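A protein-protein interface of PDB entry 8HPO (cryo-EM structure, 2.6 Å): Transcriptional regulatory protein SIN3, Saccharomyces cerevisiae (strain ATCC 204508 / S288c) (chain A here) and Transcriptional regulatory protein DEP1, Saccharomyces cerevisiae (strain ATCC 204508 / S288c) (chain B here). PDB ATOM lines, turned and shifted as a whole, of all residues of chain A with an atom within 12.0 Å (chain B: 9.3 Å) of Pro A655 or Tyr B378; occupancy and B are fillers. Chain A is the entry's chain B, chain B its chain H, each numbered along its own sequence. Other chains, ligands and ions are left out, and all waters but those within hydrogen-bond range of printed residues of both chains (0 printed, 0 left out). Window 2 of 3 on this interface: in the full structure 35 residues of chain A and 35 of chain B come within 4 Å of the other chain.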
ATOM      1  N   GLU A 651     -30.212  16.016  29.876  1.00  0.00           N
ATOM      2  CA  GLU A 651     -30.196  17.194  29.029  1.00  0.00           C
ATOM      3  C   GLU A 651     -29.386  16.898  27.770  1.00  0.00           C
ATOM      4  O   GLU A 651     -28.627  15.925  27.736  1.00  0.00           O
ATOM      5  CB  GLU A 651     -29.600  18.376  29.790  1.00  0.00           C
ATOM      6  CG  GLU A 651     -30.083  18.492  31.223  1.00  0.00           C
ATOM      7  CD  GLU A 651     -29.408  17.503  32.144  1.00  0.00           C
ATOM      8  OE1 GLU A 651     -28.489  16.800  31.677  1.00  0.00           O
ATOM      9  OE2 GLU A 651     -29.806  17.415  33.324  1.00  0.00           O
ATOM     10  N   PRO A 652     -29.535  17.706  26.704  1.00  0.00           N
ATOM     11  CA  PRO A 652     -28.913  17.329  25.428  1.00  0.00           C
ATOM     12  C   PRO A 652     -27.409  17.146  25.520  1.00  0.00           C
ATOM     13  O   PRO A 652     -26.911  16.040  25.292  1.00  0.00           O
ATOM     14  CB  PRO A 652     -29.283  18.496  24.505  1.00  0.00           C
ATOM     15  CG  PRO A 652     -30.562  18.998  25.059  1.00  0.00           C
ATOM     16  CD  PRO A 652     -30.393  18.895  26.550  1.00  0.00           C
ATOM     17  N   THR A 653     -26.681  18.203  25.864  1.00  0.00           N
ATOM     18  CA  THR A 653     -25.238  18.169  26.064  1.00  0.00           C
ATOM     19  C   THR A 653     -24.801  19.579  26.433  1.00  0.00           C
ATOM     20  O   THR A 653     -25.519  20.550  26.179  1.00  0.00           O
ATOM     21  CB  THR A 653     -24.488  17.680  24.811  1.00  0.00           C
ATOM     22  OG1 THR A 653     -24.937  16.368  24.456  1.00  0.00           O
ATOM     23  CG2 THR A 653     -23.005  17.616  25.045  1.00  0.00           C
ATOM     24  N   GLU A 654     -23.616  19.683  27.032  1.00  0.00           N
ATOM     25  CA  GLU A 654     -22.922  20.950  27.175  1.00  0.00           C
ATOM     26  C   GLU A 654     -21.843  21.035  26.110  1.00  0.00           C
ATOM     27  O   GLU A 654     -20.980  20.149  26.046  1.00  0.00           O
ATOM     28  CB  GLU A 654     -22.313  21.084  28.568  1.00  0.00           C
ATOM     29  CG  GLU A 654     -23.317  20.964  29.703  1.00  0.00           C
ATOM     30  CD  GLU A 654     -24.158  22.215  29.899  1.00  0.00           C
ATOM     31  OE1 GLU A 654     -24.493  22.891  28.904  1.00  0.00           O
ATOM     32  OE2 GLU A 654     -24.489  22.523  31.061  1.00  0.00           O
ATOM     33  N   PRO A 655     -21.862  22.051  25.251  1.00  0.00           N
ATOM     34  CA  PRO A 655     -20.842  22.155  24.204  1.00  0.00           C
ATOM     35  C   PRO A 655     -19.461  22.348  24.800  1.00  0.00           C
ATOM     36  O   PRO A 655     -19.293  22.852  25.911  1.00  0.00           O
ATOM     37  CB  PRO A 655     -21.274  23.386  23.399  1.00  0.00           C
ATOM     38  CG  PRO A 655     -22.712  23.586  23.735  1.00  0.00           C
ATOM     39  CD  PRO A 655     -22.862  23.125  25.152  1.00  0.00           C
ATOM     40  N   ILE A 656     -18.456  21.940  24.026  1.00  0.00           N
ATOM     41  CA  ILE A 656     -17.091  21.985  24.513  1.00  0.00           C
ATOM     42  C   ILE A 656     -16.663  23.431  24.748  1.00  0.00           C
ATOM     43  O   ILE A 656     -17.307  24.384  24.300  1.00  0.00           O
ATOM     44  CB  ILE A 656     -16.154  21.285  23.521  1.00  0.00           C
ATOM     45  CG1 ILE A 656     -16.927  20.231  22.741  1.00  0.00           C
ATOM     46  CG2 ILE A 656     -15.001  20.631  24.248  1.00  0.00           C
ATOM     47  CD1 ILE A 656     -16.101  19.559  21.697  1.00  0.00           C
ATOM     48  N   GLU A 657     -15.565  23.591  25.483  1.00  0.00           N
ATOM     49  CA  GLU A 657     -15.056  24.908  25.835  1.00  0.00           C
ATOM     50  C   GLU A 657     -14.390  25.629  24.677  1.00  0.00           C
ATOM     51  O   GLU A 657     -14.537  26.849  24.567  1.00  0.00           O
ATOM     52  CB  GLU A 657     -14.060  24.805  26.992  1.00  0.00           C
ATOM     53  CG  GLU A 657     -14.627  25.242  28.328  1.00  0.00           C
ATOM     54  CD  GLU A 657     -15.726  26.274  28.183  1.00  0.00           C
ATOM     55  OE1 GLU A 657     -16.908  25.917  28.374  1.00  0.00           O
ATOM     56  OE2 GLU A 657     -15.412  27.444  27.878  1.00  0.00           O
ATOM     57  N   ASN A 658     -13.684  24.919  23.803  1.00  0.00           N
ATOM     58  CA  ASN A 658     -12.901  25.568  22.763  1.00  0.00           C
ATOM     59  C   ASN A 658     -13.743  25.986  21.571  1.00  0.00           C
ATOM     60  O   ASN A 658     -13.205  26.158  20.473  1.00  0.00           O
ATOM     61  CB  ASN A 658     -11.748  24.663  22.317  1.00  0.00           C
ATOM     62  CG  ASN A 658     -12.218  23.388  21.656  1.00  0.00           C
ATOM     63  OD1 ASN A 658     -12.810  23.412  20.580  1.00  0.00           O
ATOM     64  ND2 ASN A 658     -11.946  22.258  22.296  1.00  0.00           N
ATOM     65  N   ASN A 659     -15.053  26.129  21.756  1.00  0.00           N
ATOM     66  CA  ASN A 659     -15.935  26.625  20.712  1.00  0.00           C
ATOM     67  C   ASN A 659     -16.423  28.048  20.934  1.00  0.00           C
ATOM     68  O   ASN A 659     -16.846  28.689  19.972  1.00  0.00           O
ATOM     69  CB  ASN A 659     -17.155  25.707  20.571  1.00  0.00           C
ATOM     70  CG  ASN A 659     -16.778  24.286  20.215  1.00  0.00           C
ATOM     71  OD1 ASN A 659     -15.616  23.901  20.309  1.00  0.00           O
ATOM     72  ND2 ASN A 659     -17.762  23.495  19.808  1.00  0.00           N
ATOM     73  N   ILE A 660     -16.399  28.560  22.166  1.00  0.00           N
ATOM     74  CA  ILE A 660     -17.057  29.832  22.463  1.00  0.00           C
ATOM     75  C   ILE A 660     -16.120  30.814  23.167  1.00  0.00           C
ATOM     76  O   ILE A 660     -16.563  31.624  23.988  1.00  0.00           O
ATOM     77  CB  ILE A 660     -18.342  29.619  23.291  1.00  0.00           C
ATOM     78  CG1 ILE A 660     -19.081  28.345  22.872  1.00  0.00           C
ATOM     79  CG2 ILE A 660     -19.305  30.783  23.097  1.00  0.00           C
ATOM     80  CD1 ILE A 660     -18.701  27.114  23.661  1.00  0.00           C
ATOM     81  N   SER A 661     -14.819  30.751  22.881  1.00  0.00           N
ATOM     82  CA  SER A 661     -13.852  31.684  23.473  1.00  0.00           C
ATOM     83  C   SER A 661     -13.018  32.311  22.356  1.00  0.00           C
ATOM     84  O   SER A 661     -12.010  31.735  21.938  1.00  0.00           O
ATOM     85  CB  SER A 661     -12.968  30.971  24.498  1.00  0.00           C
ATOM     86  OG  SER A 661     -13.733  30.130  25.342  1.00  0.00           O
ATOM     87  N   SER B 370     -25.582  12.310  30.184  1.00  0.00           N
ATOM     88  CA  SER B 370     -25.473  13.383  29.204  1.00  0.00           C
ATOM     89  C   SER B 370     -24.023  13.646  28.831  1.00  0.00           C
ATOM     90  O   SER B 370     -23.721  13.920  27.666  1.00  0.00           O
ATOM     91  CB  SER B 370     -26.123  14.652  29.737  1.00  0.00           C
ATOM     92  OG  SER B 370     -25.430  15.792  29.280  1.00  0.00           O
ATOM     93  N   ASP B 371     -23.109  13.570  29.798  1.00  0.00           N
ATOM     94  CA  ASP B 371     -21.695  13.735  29.465  1.00  0.00           C
ATOM     95  C   ASP B 371     -21.219  12.644  28.516  1.00  0.00           C
ATOM     96  O   ASP B 371     -20.454  12.916  27.583  1.00  0.00           O
ATOM     97  CB  ASP B 371     -20.842  13.748  30.730  1.00  0.00           C
ATOM     98  CG  ASP B 371     -20.675  15.139  31.311  1.00  0.00           C
ATOM     99  OD1 ASP B 371     -21.668  15.712  31.805  1.00  0.00           O
ATOM    100  OD2 ASP B 371     -19.541  15.660  31.271  1.00  0.00           O
ATOM    101  N   LEU B 372     -21.668  11.406  28.725  1.00  0.00           N
ATOM    102  CA  LEU B 372     -21.271  10.330  27.812  1.00  0.00           C
ATOM    103  C   LEU B 372     -21.815  10.556  26.402  1.00  0.00           C
ATOM    104  O   LEU B 372     -21.076  10.451  25.409  1.00  0.00           O
ATOM    105  CB  LEU B 372     -21.744   8.985  28.351  1.00  0.00           C
ATOM    106  CG  LEU B 372     -21.030   8.493  29.602  1.00  0.00           C
ATOM    107  CD1 LEU B 372     -21.663   7.215  30.093  1.00  0.00           C
ATOM    108  CD2 LEU B 372     -19.556   8.295  29.316  1.00  0.00           C
ATOM    109  N   GLU B 373     -23.101  10.885  26.291  1.00  0.00           N
ATOM    110  CA  GLU B 373     -23.680  11.068  24.965  1.00  0.00           C
ATOM    111  C   GLU B 373     -23.113  12.311  24.291  1.00  0.00           C
ATOM    112  O   GLU B 373     -23.055  12.395  23.060  1.00  0.00           O
ATOM    113  CB  GLU B 373     -25.205  11.134  25.048  1.00  0.00           C
ATOM    114  CG  GLU B 373     -25.765  12.413  25.607  1.00  0.00           C
ATOM    115  CD  GLU B 373     -27.140  12.715  25.055  1.00  0.00           C
ATOM    116  OE1 GLU B 373     -27.432  12.269  23.928  1.00  0.00           O
ATOM    117  OE2 GLU B 373     -27.935  13.382  25.748  1.00  0.00           O
ATOM    118  N   GLY B 374     -22.647  13.276  25.080  1.00  0.00           N
ATOM    119  CA  GLY B 374     -22.001  14.432  24.491  1.00  0.00           C
ATOM    120  C   GLY B 374     -20.620  14.109  23.968  1.00  0.00           C
ATOM    121  O   GLY B 374     -20.222  14.590  22.906  1.00  0.00           O
ATOM    122  N   LEU B 375     -19.860  13.319  24.722  1.00  0.00           N
ATOM    123  CA  LEU B 375     -18.615  12.777  24.198  1.00  0.00           C
ATOM    124  C   LEU B 375     -18.855  12.109  22.854  1.00  0.00           C
ATOM    125  O   LEU B 375     -18.050  12.243  21.926  1.00  0.00           O
ATOM    126  CB  LEU B 375     -18.021  11.795  25.210  1.00  0.00           C
ATOM    127  CG  LEU B 375     -16.642  11.168  25.023  1.00  0.00           C
ATOM    128  CD1 LEU B 375     -16.160  10.644  26.346  1.00  0.00           C
ATOM    129  CD2 LEU B 375     -16.697  10.036  24.029  1.00  0.00           C
ATOM    130  N   ARG B 376     -19.990  11.417  22.721  1.00  0.00           N
ATOM    131  CA  ARG B 376     -20.293  10.768  21.445  1.00  0.00           C
ATOM    132  C   ARG B 376     -20.620  11.778  20.352  1.00  0.00           C
ATOM    133  O   ARG B 376     -20.109  11.673  19.234  1.00  0.00           O
ATOM    134  CB  ARG B 376     -21.450   9.789  21.595  1.00  0.00           C
ATOM    135  CG  ARG B 376     -21.572   8.845  20.414  1.00  0.00           C
ATOM    136  CD  ARG B 376     -23.019   8.518  20.112  1.00  0.00           C
ATOM    137  NE  ARG B 376     -23.713   9.653  19.516  1.00  0.00           N
ATOM    138  CZ  ARG B 376     -24.868  10.136  19.954  1.00  0.00           C
ATOM    139  NH1 ARG B 376     -25.468   9.581  20.994  1.00  0.00           N
ATOM    140  NH2 ARG B 376     -25.425  11.173  19.350  1.00  0.00           N
ATOM    141  N   LYS B 377     -21.486  12.749  20.639  1.00  0.00           N
ATOM    142  CA  LYS B 377     -21.970  13.633  19.582  1.00  0.00           C
ATOM    143  C   LYS B 377     -20.923  14.672  19.190  1.00  0.00           C
ATOM    144  O   LYS B 377     -21.044  15.322  18.149  1.00  0.00           O
ATOM    145  CB  LYS B 377     -23.266  14.322  20.006  1.00  0.00           C
ATOM    146  CG  LYS B 377     -23.050  15.631  20.733  1.00  0.00           C
ATOM    147  CD  LYS B 377     -24.355  16.337  21.054  1.00  0.00           C
ATOM    148  CE  LYS B 377     -25.261  16.442  19.840  1.00  0.00           C
ATOM    149  NZ  LYS B 377     -24.556  16.985  18.648  1.00  0.00           N
ATOM    150  N   TYR B 378     -19.894  14.862  20.019  1.00  0.00           N
ATOM    151  CA  TYR B 378     -18.876  15.854  19.695  1.00  0.00           C
ATOM    152  C   TYR B 378     -17.533  15.264  19.302  1.00  0.00           C
ATOM    153  O   TYR B 378     -16.916  15.764  18.360  1.00  0.00           O
ATOM    154  CB  TYR B 378     -18.676  16.820  20.860  1.00  0.00           C
ATOM    155  CG  TYR B 378     -19.782  17.824  20.955  1.00  0.00           C
ATOM    156  CD1 TYR B 378     -20.186  18.525  19.835  1.00  0.00           C
ATOM    157  CD2 TYR B 378     -20.430  18.069  22.150  1.00  0.00           C
ATOM    158  CE1 TYR B 378     -21.202  19.441  19.900  1.00  0.00           C
ATOM    159  CE2 TYR B 378     -21.448  18.990  22.225  1.00  0.00           C
ATOM    160  CZ  TYR B 378     -21.828  19.672  21.095  1.00  0.00           C
ATOM    161  OH  TYR B 378     -22.844  20.590  21.156  1.00  0.00           O
ATOM    162  N   PHE B 379     -17.042  14.236  19.990  1.00  0.00           N
ATOM    163  CA  PHE B 379     -15.779  13.635  19.596  1.00  0.00           C
ATOM    164  C   PHE B 379     -15.976  12.363  18.794  1.00  0.00           C
ATOM    165  O   PHE B 379     -14.986  11.730  18.414  1.00  0.00           O
ATOM    166  CB  PHE B 379     -14.900  13.357  20.822  1.00  0.00           C
ATOM    167  CG  PHE B 379     -14.667  14.562  21.688  1.00  0.00           C
ATOM    168  CD1 PHE B 379     -13.557  15.357  21.506  1.00  0.00           C
ATOM    169  CD2 PHE B 379     -15.560  14.894  22.691  1.00  0.00           C
ATOM    170  CE1 PHE B 379     -13.347  16.459  22.296  1.00  0.00           C
ATOM    171  CE2 PHE B 379     -15.354  15.995  23.481  1.00  0.00           C
ATOM    172  CZ  PHE B 379     -14.245  16.776  23.287  1.00  0.00           C
ATOM    173  N   HIS B 380     -17.224  11.989  18.513  1.00  0.00           N
ATOM    174  CA  HIS B 380     -17.546  10.830  17.685  1.00  0.00           C
ATOM    175  C   HIS B 380     -16.781   9.601  18.155  1.00  0.00           C
ATOM    176  O   HIS B 380     -15.934   9.059  17.446  1.00  0.00           O
ATOM    177  CB  HIS B 380     -17.267  11.122  16.211  1.00  0.00           C
ATOM    178  CG  HIS B 380     -17.703  12.486  15.774  1.00  0.00           C
ATOM    179  ND1 HIS B 380     -19.028  12.850  15.687  1.00  0.00           N
ATOM    180  CD2 HIS B 380     -16.988  13.574  15.404  1.00  0.00           C
ATOM    181  CE1 HIS B 380     -19.112  14.105  15.285  1.00  0.00           C
ATOM    182  NE2 HIS B 380     -17.888  14.568  15.107  1.00  0.00           N
ATOM    183  N   SER B 381     -17.071   9.172  19.381  1.00  0.00           N
ATOM    184  CA  SER B 381     -16.294   8.125  20.022  1.00  0.00           C
ATOM    185  C   SER B 381     -17.198   7.283  20.906  1.00  0.00           C
ATOM    186  O   SER B 381     -18.360   7.616  21.151  1.00  0.00           O
ATOM    187  CB  SER B 381     -15.161   8.721  20.854  1.00  0.00           C
ATOM    188  OG  SER B 381     -14.115   9.190  20.032  1.00  0.00           O
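The backbone carbonyl oxygen of Glu A651 lies close to the side-chain carboxylate of Glu B373. The backbone carbonyl oxygen of Pro A652 lies close to the side-chain carboxylate of Glu B373 (2.9 Å).
The side-chain hydroxyl (OG) of Ser B381 is in hydrogen-bond range of the backbone carbonyl oxygen (O) of Phe B379 (3.1 Å).
Among the printed residues, merely in contact across the chains: Thr A653 with Gly B374 (3.4 Å), Glu A651 with Ser B370 (3.4 Å), Thr A653 with Lys B377 (3.5 Å), Thr A653 with Tyr B378 (3.5 Å), Ile A656 with Phe B379 (3.7 Å), Pro A655 with Tyr B378 (3.8 Å) and Ile A656 with Tyr B378 (3.9 Å).
Printed residues of chain B within 4 Å of Glu A651: Ser B370 and Glu B373. Printed residues of chain B within 4 Å of Pro A652: Glu B373. Printed residues of chain B within 4 Å of Pro A655: Tyr B378 (3.8 Å). Of chain B, only Tyr B378 (3.9 Å) and Phe B379 (3.7 Å) come within 4 Å of Ile A656. Asn A658 touches none of the printed residues of chain B. Printed residues of chain A within 4 Å of Ser B370: Glu A651 (3.4 Å). Of the printed residues of chain A, Glu B373 touches Glu A651 (3.3 Å) and Pro A652 (2.9 Å). Of the printed residues of chain A, Gly B374 touches Thr A653 (3.4 Å). Lys B377 touches just one residue of chain A: Thr A653 (3.5 Å). Tyr B378 touches just these residues of chain A: Thr A653 (3.5 Å), Pro A655 (3.8 Å) and Ile A656 (3.9 Å). Phe B379 touches one residue of chain A.
Printed residues of chain A that touch a printed residue of chain B: Glu A651, Pro A652, Thr A653, Pro A655 and Ile A656. Along chain A the printed residues that touch a printed residue of chain B span positions 651 to 656. Of the 12 printed residues of chain B, 6 touch a printed residue of chain A. Printed residues of chain B that touch a printed residue of chain A: Ser B370, Glu B373, Gly B374, Lys B377, Tyr B378 and Phe B379. Hydrophobic or aromatic side chains of chain B within 4 Å of the printed part of chain A: Tyr B378 and Phe B379. Among the printed residues, 9 pairs touch across the chains. Among the printed residues, no Asp or Glu carboxylate lies within 4 Å of a Lys or Arg side-chain nitrogen of the other chain.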
